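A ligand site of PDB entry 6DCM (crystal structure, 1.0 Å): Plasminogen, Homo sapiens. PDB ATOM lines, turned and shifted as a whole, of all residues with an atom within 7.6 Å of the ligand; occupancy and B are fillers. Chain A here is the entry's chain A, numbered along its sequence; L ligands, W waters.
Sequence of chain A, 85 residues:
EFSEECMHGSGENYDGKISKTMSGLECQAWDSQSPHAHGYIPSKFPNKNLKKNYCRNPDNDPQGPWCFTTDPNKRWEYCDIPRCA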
ATOM      1  N   HIS A  36     -15.421   2.974 -15.577  1.00  0.00           N
ATOM      2  CA  HIS A  36     -14.154   3.474 -16.118  1.00  0.00           C
ATOM      3  C   HIS A  36     -14.283   4.935 -16.532  1.00  0.00           C
ATOM      4  O   HIS A  36     -15.164   5.278 -17.322  1.00  0.00           O
ATOM      5  CB  HIS A  36     -13.719   2.611 -17.289  1.00  0.00           C
ATOM      6  CG  HIS A  36     -13.700   1.170 -16.914  1.00  0.00           C
ATOM      7  ND1 HIS A  36     -12.816   0.668 -15.987  1.00  0.00           N
ATOM      8  CD2 HIS A  36     -14.533   0.153 -17.245  1.00  0.00           C
ATOM      9  CE1 HIS A  36     -13.070  -0.614 -15.795  1.00  0.00           C
ATOM     10  NE2 HIS A  36     -14.105  -0.944 -16.543  1.00  0.00           N
ATOM     11  N   ALA A  37     -13.400   5.765 -15.982  1.00  0.00           N
ATOM     12  CA  ALA A  37     -13.313   7.164 -16.369  1.00  0.00           C
ATOM     13  C   ALA A  37     -12.484   7.273 -17.639  1.00  0.00           C
ATOM     14  O   ALA A  37     -11.512   6.535 -17.833  1.00  0.00           O
ATOM     15  CB  ALA A  37     -12.679   7.987 -15.252  1.00  0.00           C
ATOM     16  N   HIS A  38     -12.865   8.189 -18.528  1.00  0.00           N
ATOM     17  CA  HIS A  38     -12.231   8.216 -19.837  1.00  0.00           C
ATOM     18  C   HIS A  38     -12.490   9.555 -20.517  1.00  0.00           C
ATOM     19  O   HIS A  38     -13.341  10.346 -20.102  1.00  0.00           O
ATOM     20  CB  HIS A  38     -12.751   7.082 -20.710  1.00  0.00           C
ATOM     21  CG  HIS A  38     -14.186   7.259 -21.088  1.00  0.00           C
ATOM     22  ND1 HIS A  38     -14.577   7.945 -22.209  1.00  0.00           N
ATOM     23  CD2 HIS A  38     -15.322   6.877 -20.448  1.00  0.00           C
ATOM     24  CE1 HIS A  38     -15.901   7.960 -22.257  1.00  0.00           C
ATOM     25  NE2 HIS A  38     -16.372   7.312 -21.210  1.00  0.00           N
ATOM     26  N   GLY A  39     -11.750   9.779 -21.609  1.00  0.00           N
ATOM     27  CA  GLY A  39     -11.835  11.006 -22.371  1.00  0.00           C
ATOM     28  C   GLY A  39     -12.439  10.888 -23.761  1.00  0.00           C
ATOM     29  O   GLY A  39     -12.256  11.797 -24.585  1.00  0.00           O
ATOM     30  N   TYR A  40     -13.146   9.790 -24.045  1.00  0.00           N
ATOM     31  CA  TYR A  40     -13.835   9.603 -25.324  1.00  0.00           C
ATOM     32  C   TYR A  40     -15.278  10.094 -25.200  1.00  0.00           C
ATOM     33  O   TYR A  40     -16.242   9.330 -25.169  1.00  0.00           O
ATOM     34  CB  TYR A  40     -13.727   8.158 -25.791  1.00  0.00           C
ATOM     35  CG  TYR A  40     -12.329   7.899 -26.310  1.00  0.00           C
ATOM     36  CD1 TYR A  40     -11.992   8.276 -27.607  1.00  0.00           C
ATOM     37  CD2 TYR A  40     -11.342   7.365 -25.502  1.00  0.00           C
ATOM     38  CE1 TYR A  40     -10.723   8.097 -28.099  1.00  0.00           C
ATOM     39  CE2 TYR A  40     -10.055   7.163 -25.992  1.00  0.00           C
ATOM     40  CZ  TYR A  40      -9.760   7.545 -27.293  1.00  0.00           C
ATOM     41  OH  TYR A  40      -8.505   7.382 -27.810  1.00  0.00           O
ATOM     42  N   ARG A  56     -17.162   0.972 -30.840  1.00  0.00           N
ATOM     43  CA  ARG A  56     -16.676   1.974 -31.788  1.00  0.00           C
ATOM     44  C   ARG A  56     -15.155   1.956 -31.779  1.00  0.00           C
ATOM     45  O   ARG A  56     -14.526   1.344 -30.913  1.00  0.00           O
ATOM     46  CB  ARG A  56     -17.192   3.373 -31.446  1.00  0.00           C
ATOM     47  CG  ARG A  56     -18.708   3.564 -31.608  1.00  0.00           C
ATOM     48  CD  ARG A  56     -19.123   3.616 -33.072  1.00  0.00           C
ATOM     49  NE  ARG A  56     -20.555   3.854 -33.251  1.00  0.00           N
ATOM     50  CZ  ARG A  56     -21.464   2.900 -33.372  1.00  0.00           C
ATOM     51  NH1 ARG A  56     -21.111   1.615 -33.323  1.00  0.00           N
ATOM     52  NH2 ARG A  56     -22.741   3.232 -33.555  1.00  0.00           N
ATOM     53  N   ASN A  57     -14.570   2.639 -32.757  1.00  0.00           N
ATOM     54  CA  ASN A  57     -13.117   2.696 -32.896  1.00  0.00           C
ATOM     55  C   ASN A  57     -12.628   4.140 -32.968  1.00  0.00           C
ATOM     56  O   ASN A  57     -12.082   4.579 -33.984  1.00  0.00           O
ATOM     57  CB  ASN A  57     -12.654   1.901 -34.114  1.00  0.00           C
ATOM     58  CG  ASN A  57     -11.168   1.702 -34.120  1.00  0.00           C
ATOM     59  OD1 ASN A  57     -10.491   2.045 -33.143  1.00  0.00           O
ATOM     60  ND2 ASN A  57     -10.654   1.149 -35.201  1.00  0.00           N
ATOM     61  N   PRO A  58     -12.795   4.899 -31.878  1.00  0.00           N
ATOM     62  CA  PRO A  58     -12.468   6.342 -31.934  1.00  0.00           C
ATOM     63  C   PRO A  58     -10.986   6.642 -31.902  1.00  0.00           C
ATOM     64  O   PRO A  58     -10.613   7.789 -32.178  1.00  0.00           O
ATOM     65  CB  PRO A  58     -13.171   6.902 -30.692  1.00  0.00           C
ATOM     66  CG  PRO A  58     -13.219   5.753 -29.743  1.00  0.00           C
ATOM     67  CD  PRO A  58     -13.435   4.532 -30.597  1.00  0.00           C
ATOM     68  N   ASP A  59     -10.125   5.674 -31.578  1.00  0.00           N
ATOM     69  CA  ASP A  59      -8.683   5.874 -31.621  1.00  0.00           C
ATOM     70  C   ASP A  59      -8.023   5.197 -32.808  1.00  0.00           C
ATOM     71  O   ASP A  59      -6.792   5.065 -32.831  1.00  0.00           O
ATOM     72  CB  ASP A  59      -8.029   5.437 -30.303  1.00  0.00           C
ATOM     73  CG  ASP A  59      -8.039   3.946 -30.112  1.00  0.00           C
ATOM     74  OD1 ASP A  59      -8.943   3.290 -30.665  1.00  0.00           O
ATOM     75  OD2 ASP A  59      -7.147   3.432 -29.405  1.00  0.00           O
ATOM     76  N   ASN A  60      -8.798   4.760 -33.802  1.00  0.00           N
ATOM     77  CA  ASN A  60      -8.235   4.231 -35.039  1.00  0.00           C
ATOM     78  C   ASN A  60      -7.337   3.025 -34.785  1.00  0.00           C
ATOM     79  O   ASN A  60      -6.280   2.867 -35.394  1.00  0.00           O
ATOM     80  CB  ASN A  60      -7.511   5.315 -35.850  1.00  0.00           C
ATOM     81  CG  ASN A  60      -8.359   6.556 -36.041  1.00  0.00           C
ATOM     82  OD1 ASN A  60      -9.524   6.465 -36.414  1.00  0.00           O
ATOM     83  ND2 ASN A  60      -7.795   7.722 -35.743  1.00  0.00           N
ATOM     84  N   ASP A  61      -7.761   2.166 -33.867  1.00  0.00           N
ATOM     85  CA  ASP A  61      -7.011   0.949 -33.580  1.00  0.00           C
ATOM     86  C   ASP A  61      -7.079   0.029 -34.789  1.00  0.00           C
ATOM     87  O   ASP A  61      -8.184  -0.283 -35.272  1.00  0.00           O
ATOM     88  CB  ASP A  61      -7.650   0.291 -32.363  1.00  0.00           C
ATOM     89  CG  ASP A  61      -6.817  -0.841 -31.771  1.00  0.00           C
ATOM     90  OD1 ASP A  61      -6.217  -1.624 -32.548  1.00  0.00           O
ATOM     91  OD2 ASP A  61      -6.793  -0.956 -30.524  1.00  0.00           O
ATOM     92  N   PRO A  62      -5.947  -0.453 -35.313  1.00  0.00           N
ATOM     93  CA  PRO A  62      -6.022  -1.338 -36.483  1.00  0.00           C
ATOM     94  C   PRO A  62      -6.717  -2.660 -36.213  1.00  0.00           C
ATOM     95  O   PRO A  62      -7.101  -3.353 -37.171  1.00  0.00           O
ATOM     96  CB  PRO A  62      -4.545  -1.537 -36.872  1.00  0.00           C
ATOM     97  CG  PRO A  62      -3.807  -1.328 -35.617  1.00  0.00           C
ATOM     98  CD  PRO A  62      -4.564  -0.254 -34.863  1.00  0.00           C
ATOM     99  N   GLN A  63      -6.917  -3.039 -34.947  1.00  0.00           N
ATOM    100  CA  GLN A  63      -7.679  -4.239 -34.627  1.00  0.00           C
ATOM    101  C   GLN A  63      -9.184  -4.010 -34.587  1.00  0.00           C
ATOM    102  O   GLN A  63      -9.936  -4.967 -34.389  1.00  0.00           O
ATOM    103  CB  GLN A  63      -7.196  -4.868 -33.321  1.00  0.00           C
ATOM    104  CG  GLN A  63      -5.782  -5.420 -33.406  1.00  0.00           C
ATOM    105  CD  GLN A  63      -5.499  -6.356 -32.263  1.00  0.00           C
ATOM    106  OE1 GLN A  63      -5.020  -5.940 -31.201  1.00  0.00           O
ATOM    107  NE2 GLN A  63      -5.847  -7.615 -32.434  1.00  0.00           N
ATOM    108  N   GLY A  64      -9.651  -2.767 -34.743  1.00  0.00           N
ATOM    109  CA  GLY A  64     -11.065  -2.517 -34.897  1.00  0.00           C
ATOM    110  C   GLY A  64     -11.763  -2.036 -33.638  1.00  0.00           C
ATOM    111  O   GLY A  64     -11.119  -1.712 -32.618  1.00  0.00           O
ATOM    112  N   PRO A  65     -13.094  -2.013 -33.676  1.00  0.00           N
ATOM    113  CA  PRO A  65     -13.884  -1.440 -32.588  1.00  0.00           C
ATOM    114  C   PRO A  65     -13.773  -2.186 -31.266  1.00  0.00           C
ATOM    115  O   PRO A  65     -13.479  -3.392 -31.199  1.00  0.00           O
ATOM    116  CB  PRO A  65     -15.310  -1.468 -33.129  1.00  0.00           C
ATOM    117  CG  PRO A  65     -15.143  -1.445 -34.613  1.00  0.00           C
ATOM    118  CD  PRO A  65     -13.925  -2.276 -34.861  1.00  0.00           C
ATOM    119  N   TRP A  66     -14.073  -1.431 -30.211  1.00  0.00           N
ATOM    120  CA  TRP A  66     -13.899  -1.837 -28.838  1.00  0.00           C
ATOM    121  C   TRP A  66     -14.882  -1.008 -27.998  1.00  0.00           C
ATOM    122  O   TRP A  66     -15.580  -0.137 -28.503  1.00  0.00           O
ATOM    123  CB  TRP A  66     -12.448  -1.611 -28.381  1.00  0.00           C
ATOM    124  CG  TRP A  66     -11.932  -0.217 -28.657  1.00  0.00           C
ATOM    125  CD1 TRP A  66     -11.335   0.225 -29.808  1.00  0.00           C
ATOM    126  CD2 TRP A  66     -11.976   0.908 -27.761  1.00  0.00           C
ATOM    127  NE1 TRP A  66     -11.008   1.565 -29.680  1.00  0.00           N
ATOM    128  CE2 TRP A  66     -11.396   2.001 -28.444  1.00  0.00           C
ATOM    129  CE3 TRP A  66     -12.451   1.104 -26.465  1.00  0.00           C
ATOM    130  CZ2 TRP A  66     -11.272   3.259 -27.865  1.00  0.00           C
ATOM    131  CZ3 TRP A  66     -12.325   2.369 -25.879  1.00  0.00           C
ATOM    132  CH2 TRP A  66     -11.744   3.426 -26.585  1.00  0.00           C
ATOM    133  N   CYS A  67     -14.917  -1.294 -26.695  1.00  0.00           N
ATOM    134  CA  CYS A  67     -15.653  -0.433 -25.788  1.00  0.00           C
ATOM    135  C   CYS A  67     -15.015  -0.526 -24.407  1.00  0.00           C
ATOM    136  O   CYS A  67     -14.334  -1.506 -24.093  1.00  0.00           O
ATOM    137  CB  CYS A  67     -17.139  -0.798 -25.713  1.00  0.00           C
ATOM    138  SG  CYS A  67     -17.417  -2.475 -25.163  1.00  0.00           S
ATOM    139  N   PHE A  68     -15.267   0.483 -23.585  1.00  0.00           N
ATOM    140  CA  PHE A  68     -15.052   0.299 -22.153  1.00  0.00           C
ATOM    141  C   PHE A  68     -16.080  -0.699 -21.661  1.00  0.00           C
ATOM    142  O   PHE A  68     -17.200  -0.737 -22.172  1.00  0.00           O
ATOM    143  CB  PHE A  68     -15.174   1.658 -21.440  1.00  0.00           C
ATOM    144  CG  PHE A  68     -14.125   2.639 -21.881  1.00  0.00           C
ATOM    145  CD1 PHE A  68     -12.805   2.462 -21.505  1.00  0.00           C
ATOM    146  CD2 PHE A  68     -14.434   3.695 -22.714  1.00  0.00           C
ATOM    147  CE1 PHE A  68     -11.820   3.322 -21.936  1.00  0.00           C
ATOM    148  CE2 PHE A  68     -13.457   4.570 -23.142  1.00  0.00           C
ATOM    149  CZ  PHE A  68     -12.138   4.372 -22.760  1.00  0.00           C
ATOM    150  N   ARG A  75     -10.952  -2.673 -18.116  1.00  0.00           N
ATOM    151  CA  ARG A  75     -11.222  -1.321 -18.589  1.00  0.00           C
ATOM    152  C   ARG A  75     -11.854  -1.321 -19.982  1.00  0.00           C
ATOM    153  O   ARG A  75     -12.860  -0.644 -20.205  1.00  0.00           O
ATOM    154  CB  ARG A  75      -9.935  -0.506 -18.554  1.00  0.00           C
ATOM    155  CG  ARG A  75     -10.107   0.913 -19.040  1.00  0.00           C
ATOM    156  CD  ARG A  75      -8.848   1.743 -18.780  1.00  0.00           C
ATOM    157  NE  ARG A  75      -8.953   3.063 -19.410  1.00  0.00           N
ATOM    158  CZ  ARG A  75      -9.619   4.093 -18.904  1.00  0.00           C
ATOM    159  NH1 ARG A  75     -10.252   4.004 -17.736  1.00  0.00           N
ATOM    160  NH2 ARG A  75      -9.676   5.229 -19.589  1.00  0.00           N
ATOM    161  N   TRP A  76     -11.264  -2.057 -20.915  1.00  0.00           N
ATOM    162  CA  TRP A  76     -11.767  -2.074 -22.281  1.00  0.00           C
ATOM    163  C   TRP A  76     -11.508  -3.436 -22.896  1.00  0.00           C
ATOM    164  O   TRP A  76     -10.689  -4.223 -22.402  1.00  0.00           O
ATOM    165  CB  TRP A  76     -11.126  -0.979 -23.145  1.00  0.00           C
ATOM    166  CG  TRP A  76      -9.646  -1.146 -23.322  1.00  0.00           C
ATOM    167  CD1 TRP A  76      -8.661  -0.639 -22.526  1.00  0.00           C
ATOM    168  CD2 TRP A  76      -8.986  -1.882 -24.351  1.00  0.00           C
ATOM    169  NE1 TRP A  76      -7.420  -1.007 -22.998  1.00  0.00           N
ATOM    170  CE2 TRP A  76      -7.596  -1.780 -24.125  1.00  0.00           C
ATOM    171  CE3 TRP A  76      -9.433  -2.615 -25.464  1.00  0.00           C
ATOM    172  CZ2 TRP A  76      -6.655  -2.376 -24.959  1.00  0.00           C
ATOM    173  CZ3 TRP A  76      -8.499  -3.210 -26.282  1.00  0.00           C
ATOM    174  CH2 TRP A  76      -7.120  -3.086 -26.030  1.00  0.00           C
ATOM    175  N   GLU A  77     -12.217  -3.716 -23.993  1.00  0.00           N
ATOM    176  CA  GLU A  77     -12.044  -4.952 -24.727  1.00  0.00           C
ATOM    177  C   GLU A  77     -12.537  -4.755 -26.159  1.00  0.00           C
ATOM    178  O   GLU A  77     -13.493  -4.006 -26.383  1.00  0.00           O
ATOM    179  CB  GLU A  77     -12.799  -6.109 -24.050  1.00  0.00           C
ATOM    180  CG  GLU A  77     -12.476  -7.480 -24.608  1.00  0.00           C
ATOM    181  CD  GLU A  77     -13.345  -8.579 -24.004  1.00  0.00           C
ATOM    182  OE1 GLU A  77     -13.298  -9.702 -24.544  1.00  0.00           O
ATOM    183  OE2 GLU A  77     -14.062  -8.334 -23.012  1.00  0.00           O
ATOM    184  N   TYR A  78     -11.869  -5.415 -27.106  1.00  0.00           N
ATOM    185  CA  TYR A  78     -12.384  -5.437 -28.477  1.00  0.00           C
ATOM    186  C   TYR A  78     -13.743  -6.108 -28.540  1.00  0.00           C
ATOM    187  O   TYR A  78     -14.079  -6.984 -27.723  1.00  0.00           O
ATOM    188  CB  TYR A  78     -11.426  -6.169 -29.430  1.00  0.00           C
ATOM    189  CG  TYR A  78     -10.106  -5.462 -29.546  1.00  0.00           C
ATOM    190  CD1 TYR A  78     -10.029  -4.180 -30.089  1.00  0.00           C
ATOM    191  CD2 TYR A  78      -8.954  -6.047 -29.062  1.00  0.00           C
ATOM    192  CE1 TYR A  78      -8.816  -3.511 -30.160  1.00  0.00           C
ATOM    193  CE2 TYR A  78      -7.743  -5.391 -29.133  1.00  0.00           C
ATOM    194  CZ  TYR A  78      -7.687  -4.122 -29.672  1.00  0.00           C
ATOM    195  OH  TYR A  78      -6.481  -3.472 -29.720  1.00  0.00           O
HETATM  196  C1  LIG L   1      -8.240   4.429 -22.763  1.00  0.00           C
HETATM  197  O1  LIG L   1      -8.902   5.454 -22.455  1.00  0.00           O
HETATM  198  O2  LIG L   1      -7.830   3.659 -21.868  1.00  0.00           O
HETATM  199  C2  LIG L   1      -7.954   4.131 -24.238  1.00  0.00           C
HETATM  200  C3  LIG L   1      -8.209   2.649 -24.513  1.00  0.00           C
HETATM  201  C4  LIG L   1      -8.022   2.349 -26.009  1.00  0.00           C
HETATM  202  C5  LIG L   1      -8.217   0.844 -26.197  1.00  0.00           C
HETATM  203  C6  LIG L   1      -8.284   0.426 -27.660  1.00  0.00           C
HETATM  204  N1  LIG L   1      -7.110   0.833 -28.410  1.00  0.00           N
HETATM  205  O   HOH W   1      -6.490   7.442 -23.415  1.00  0.00           O
HETATM  206  O   HOH W   2      -9.493   8.016 -22.059  1.00  0.00           O
HETATM  207  O   HOH W   3      -5.399   4.745 -21.812  1.00  0.00           O
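An oxygen (O2) of the ligand lies within salt-bridge range of the guanidinium group of Arg 75, at 2.8 Å.
N1 of the ligand is in salt-bridge range of OD2 of Asp 59 (2.8 Å).
The side-chain carboxylate (OD2) of Asp 61 lies within salt-bridge range of a nitrogen (N1) of the ligand (2.8 Å).
NH1 of Arg 75 is in hydrogen-bond range of O of Ala 37 (2.8 Å).
NE1 of Trp 66 lies within hydrogen-bond range of OD1 of Asp 59.
The side-chain carboxylate of Asp 59 lies close to the side-chain amide oxygen of Asn 57, at 3.2 Å.
The side-chain carboxylate of Asp 61 lies within hydrogen-bond range of the side-chain hydroxyl of Tyr 78.
The backbone NH of Asp 61 sits at hydrogen-bond distance from the side-chain amide oxygen of Asn 57 (2.8 Å).
The side-chain carboxylate (OD1) of Asp 61 is in hydrogen-bond range of the backbone NH (N) of Gln 63, 2.9 Å away.
The backbone NH (N) of Trp 66 sits at hydrogen-bond distance from the backbone carbonyl oxygen (O) of Arg 56 (2.9 Å).
Trp 66 touches the ligand.
Phe 68 touches the ligand.
Trp 76 touches the ligand (CD2 to C5, 3.4 Å).
Of the 22 residues printed, 6 come within 4 Å of the ligand.
Water W2 lies within hydrogen-bond range of an oxygen (O1) of the ligand and the backbone NH (N) of Gly 39.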
